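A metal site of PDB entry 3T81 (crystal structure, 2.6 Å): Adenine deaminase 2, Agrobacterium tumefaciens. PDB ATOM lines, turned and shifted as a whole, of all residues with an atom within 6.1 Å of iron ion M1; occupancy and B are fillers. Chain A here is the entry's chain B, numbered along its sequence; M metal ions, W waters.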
ATOM      1  N   HIS A  95      21.904 -35.422  29.104  1.00  0.00           N
ATOM      2  CA  HIS A  95      21.975 -34.122  28.448  1.00  0.00           C
ATOM      3  C   HIS A  95      20.834 -33.329  28.917  1.00  0.00           C
ATOM      4  O   HIS A  95      19.681 -33.717  28.642  1.00  0.00           O
ATOM      5  CB  HIS A  95      21.797 -34.290  26.939  1.00  0.00           C
ATOM      6  CG  HIS A  95      21.677 -32.982  26.246  1.00  0.00           C
ATOM      7  ND1 HIS A  95      22.764 -32.233  25.895  1.00  0.00           N
ATOM      8  CD2 HIS A  95      20.591 -32.222  25.973  1.00  0.00           C
ATOM      9  CE1 HIS A  95      22.377 -31.089  25.380  1.00  0.00           C
ATOM     10  NE2 HIS A  95      21.063 -31.044  25.438  1.00  0.00           N
ATOM     11  N   MET A  96      21.065 -32.237  29.632  1.00  0.00           N
ATOM     12  CA  MET A  96      19.910 -31.400  29.979  1.00  0.00           C
ATOM     13  C   MET A  96      20.111 -29.935  30.358  1.00  0.00           C
ATOM     14  O   MET A  96      21.251 -29.458  30.363  1.00  0.00           O
ATOM     15  CB  MET A  96      18.840 -32.082  30.862  1.00  0.00           C
ATOM     16  CG  MET A  96      19.314 -32.625  32.128  1.00  0.00           C
ATOM     17  SD  MET A  96      20.119 -31.224  33.275  1.00  0.00           S
ATOM     18  CE  MET A  96      18.469 -30.707  34.256  1.00  0.00           C
ATOM     19  N   HIS A  97      18.988 -29.247  30.641  1.00  0.00           N
ATOM     20  CA  HIS A  97      19.036 -27.819  30.854  1.00  0.00           C
ATOM     21  C   HIS A  97      18.132 -27.371  32.057  1.00  0.00           C
ATOM     22  O   HIS A  97      16.957 -27.063  31.851  1.00  0.00           O
ATOM     23  CB  HIS A  97      18.640 -27.076  29.597  1.00  0.00           C
ATOM     24  CG  HIS A  97      19.322 -27.546  28.349  1.00  0.00           C
ATOM     25  ND1 HIS A  97      20.688 -27.348  28.113  1.00  0.00           N
ATOM     26  CD2 HIS A  97      18.810 -28.122  27.234  1.00  0.00           C
ATOM     27  CE1 HIS A  97      20.969 -27.797  26.899  1.00  0.00           C
ATOM     28  NE2 HIS A  97      19.858 -28.283  26.347  1.00  0.00           N
ATOM     29  N   ASP A 123      24.270 -29.137  30.382  1.00  0.00           N
ATOM     30  CA  ASP A 123      24.734 -28.013  29.577  1.00  0.00           C
ATOM     31  C   ASP A 123      24.008 -26.632  30.000  1.00  0.00           C
ATOM     32  O   ASP A 123      22.827 -26.456  29.745  1.00  0.00           O
ATOM     33  CB  ASP A 123      24.308 -28.341  28.190  1.00  0.00           C
ATOM     34  CG  ASP A 123      24.597 -27.243  27.319  1.00  0.00           C
ATOM     35  OD1 ASP A 123      25.192 -26.343  27.996  1.00  0.00           O
ATOM     36  OD2 ASP A 123      24.270 -27.232  26.068  1.00  0.00           O
ATOM     37  N   HIS A 125      24.205 -23.761  28.959  1.00  0.00           N
ATOM     38  CA  HIS A 125      24.532 -22.680  28.072  1.00  0.00           C
ATOM     39  C   HIS A 125      23.548 -21.558  28.226  1.00  0.00           C
ATOM     40  O   HIS A 125      23.789 -20.519  27.739  1.00  0.00           O
ATOM     41  CB  HIS A 125      24.628 -23.169  26.630  1.00  0.00           C
ATOM     42  CG  HIS A 125      23.366 -23.624  26.032  1.00  0.00           C
ATOM     43  ND1 HIS A 125      23.208 -24.891  25.524  1.00  0.00           N
ATOM     44  CD2 HIS A 125      22.237 -22.951  25.739  1.00  0.00           C
ATOM     45  CE1 HIS A 125      22.004 -24.999  24.952  1.00  0.00           C
ATOM     46  NE2 HIS A 125      21.386 -23.834  25.109  1.00  0.00           N
ATOM     47  N   GLU A 126      22.421 -21.753  28.863  1.00  0.00           N
ATOM     48  CA  GLU A 126      21.378 -20.760  28.801  1.00  0.00           C
ATOM     49  C   GLU A 126      21.871 -19.622  29.720  1.00  0.00           C
ATOM     50  O   GLU A 126      22.125 -18.529  29.256  1.00  0.00           O
ATOM     51  CB  GLU A 126      19.981 -21.275  29.210  1.00  0.00           C
ATOM     52  CG  GLU A 126      19.507 -22.645  28.683  1.00  0.00           C
ATOM     53  CD  GLU A 126      19.129 -22.726  27.154  1.00  0.00           C
ATOM     54  OE1 GLU A 126      18.487 -21.836  26.606  1.00  0.00           O
ATOM     55  OE2 GLU A 126      19.504 -23.709  26.480  1.00  0.00           O
ATOM     56  N   GLU A 190      26.845 -29.510  24.114  1.00  0.00           N
ATOM     57  CA  GLU A 190      26.127 -29.613  22.877  1.00  0.00           C
ATOM     58  C   GLU A 190      26.656 -28.698  21.795  1.00  0.00           C
ATOM     59  O   GLU A 190      26.371 -27.530  21.776  1.00  0.00           O
ATOM     60  CB  GLU A 190      24.637 -29.291  23.221  1.00  0.00           C
ATOM     61  CG  GLU A 190      23.783 -29.183  21.997  1.00  0.00           C
ATOM     62  CD  GLU A 190      22.402 -28.881  22.321  1.00  0.00           C
ATOM     63  OE1 GLU A 190      22.304 -28.354  23.434  1.00  0.00           O
ATOM     64  OE2 GLU A 190      21.485 -29.199  21.517  1.00  0.00           O
ATOM     65  N   HIS A 242      21.396 -35.638  20.365  1.00  0.00           N
ATOM     66  CA  HIS A 242      20.011 -35.889  20.871  1.00  0.00           C
ATOM     67  C   HIS A 242      18.900 -35.614  19.920  1.00  0.00           C
ATOM     68  O   HIS A 242      17.724 -36.110  20.160  1.00  0.00           O
ATOM     69  CB  HIS A 242      19.686 -35.056  22.114  1.00  0.00           C
ATOM     70  CG  HIS A 242      20.397 -33.757  22.158  1.00  0.00           C
ATOM     71  ND1 HIS A 242      21.380 -33.500  23.089  1.00  0.00           N
ATOM     72  CD2 HIS A 242      20.360 -32.712  21.328  1.00  0.00           C
ATOM     73  CE1 HIS A 242      21.871 -32.289  22.868  1.00  0.00           C
ATOM     74  NE2 HIS A 242      21.264 -31.788  21.810  1.00  0.00           N
ATOM     75  N   GLU A 243      19.255 -34.806  18.880  1.00  0.00           N
ATOM     76  CA  GLU A 243      18.290 -34.250  17.873  1.00  0.00           C
ATOM     77  C   GLU A 243      17.966 -35.354  16.880  1.00  0.00           C
ATOM     78  O   GLU A 243      18.667 -35.456  15.887  1.00  0.00           O
ATOM     79  CB  GLU A 243      18.850 -33.040  17.156  1.00  0.00           C
ATOM     80  CG  GLU A 243      19.450 -31.990  18.036  1.00  0.00           C
ATOM     81  CD  GLU A 243      18.392 -31.027  18.702  1.00  0.00           C
ATOM     82  OE1 GLU A 243      17.183 -31.034  18.223  1.00  0.00           O
ATOM     83  OE2 GLU A 243      18.797 -30.292  19.699  1.00  0.00           O
ATOM     84  N   ARG A 263      16.259 -38.389  23.943  1.00  0.00           N
ATOM     85  CA  ARG A 263      15.385 -37.448  24.606  1.00  0.00           C
ATOM     86  C   ARG A 263      13.855 -37.724  24.771  1.00  0.00           C
ATOM     87  O   ARG A 263      13.196 -38.145  23.869  1.00  0.00           O
ATOM     88  CB  ARG A 263      15.711 -35.987  24.242  1.00  0.00           C
ATOM     89  CG  ARG A 263      15.069 -35.435  22.957  1.00  0.00           C
ATOM     90  CD  ARG A 263      15.709 -34.071  22.519  1.00  0.00           C
ATOM     91  NE  ARG A 263      15.325 -33.945  21.143  1.00  0.00           N
ATOM     92  CZ  ARG A 263      15.506 -32.892  20.339  1.00  0.00           C
ATOM     93  NH1 ARG A 263      16.176 -31.805  20.786  1.00  0.00           N
ATOM     94  NH2 ARG A 263      15.074 -32.993  19.058  1.00  0.00           N
ATOM     95  N   ASP A 292      16.871 -33.213  28.370  1.00  0.00           N
ATOM     96  CA  ASP A 292      17.006 -32.027  27.447  1.00  0.00           C
ATOM     97  C   ASP A 292      16.097 -30.871  28.004  1.00  0.00           C
ATOM     98  O   ASP A 292      16.470 -30.193  28.936  1.00  0.00           O
ATOM     99  CB  ASP A 292      16.632 -32.325  25.962  1.00  0.00           C
ATOM    100  CG  ASP A 292      17.271 -31.377  24.986  1.00  0.00           C
ATOM    101  OD1 ASP A 292      18.033 -30.525  25.406  1.00  0.00           O
ATOM    102  OD2 ASP A 292      17.046 -31.444  23.724  1.00  0.00           O
ATOM    103  N   ASP A 293      14.944 -30.606  27.426  1.00  0.00           N
ATOM    104  CA  ASP A 293      14.151 -29.412  27.956  1.00  0.00           C
ATOM    105  C   ASP A 293      12.802 -29.843  28.416  1.00  0.00           C
ATOM    106  O   ASP A 293      12.014 -30.283  27.474  1.00  0.00           O
ATOM    107  CB  ASP A 293      13.826 -28.293  26.903  1.00  0.00           C
ATOM    108  CG  ASP A 293      14.848 -28.213  25.852  1.00  0.00           C
ATOM    109  OD1 ASP A 293      14.566 -28.858  24.760  1.00  0.00           O
ATOM    110  OD2 ASP A 293      15.922 -27.620  26.170  1.00  0.00           O
HETATM  111 FE    FE M   1      19.879 -29.444  24.800  1.00  0.00          FE
HETATM  112 FE    FE M   2      20.131 -29.574  20.874  1.00  0.00          FE
HETATM  113  O   HOH W   1      19.043 -29.648  22.925  1.00  0.00           O
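A ring nitrogen (ND1) of His 97 is in hydrogen-bond range of the backbone carbonyl oxygen (O) of Asp 123, 2.8 Å away.
ND1 of His 242 lies close to ND1 of His 95, at 3.4 Å.
The side-chain carboxylate of Asp 292 is in salt-bridge range of the guanidinium group of Arg 263 (3.1 Å).
NE2 of His 242 sits close to OE2 of Glu 190 (2.6 Å).
The backbone carbonyl oxygen (O) of His 242 sits at hydrogen-bond distance from the guanidinium group (NE) of Arg 263 (3.4 Å).
Merely in contact with iron ion M1: Glu 190 (3.0 Å) and His 242 (3.97 Å).
The nearest printed residue that does not touch iron ion M1 is Asp 293 (4.6 Å).
Iron ion M1 is bound by NE2 of His 97 (1.9 Å), water W1 (2.1 Å), NE2 of His 95 (2.1 Å) and OD1 of Asp 292 (2.2 Å).
Iron ion M1 has four donor atoms within binding distance.
Water W1 bridges OD2 of Asp 292 (2.8 Å) and NE2 of His 242 (3.3 Å).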
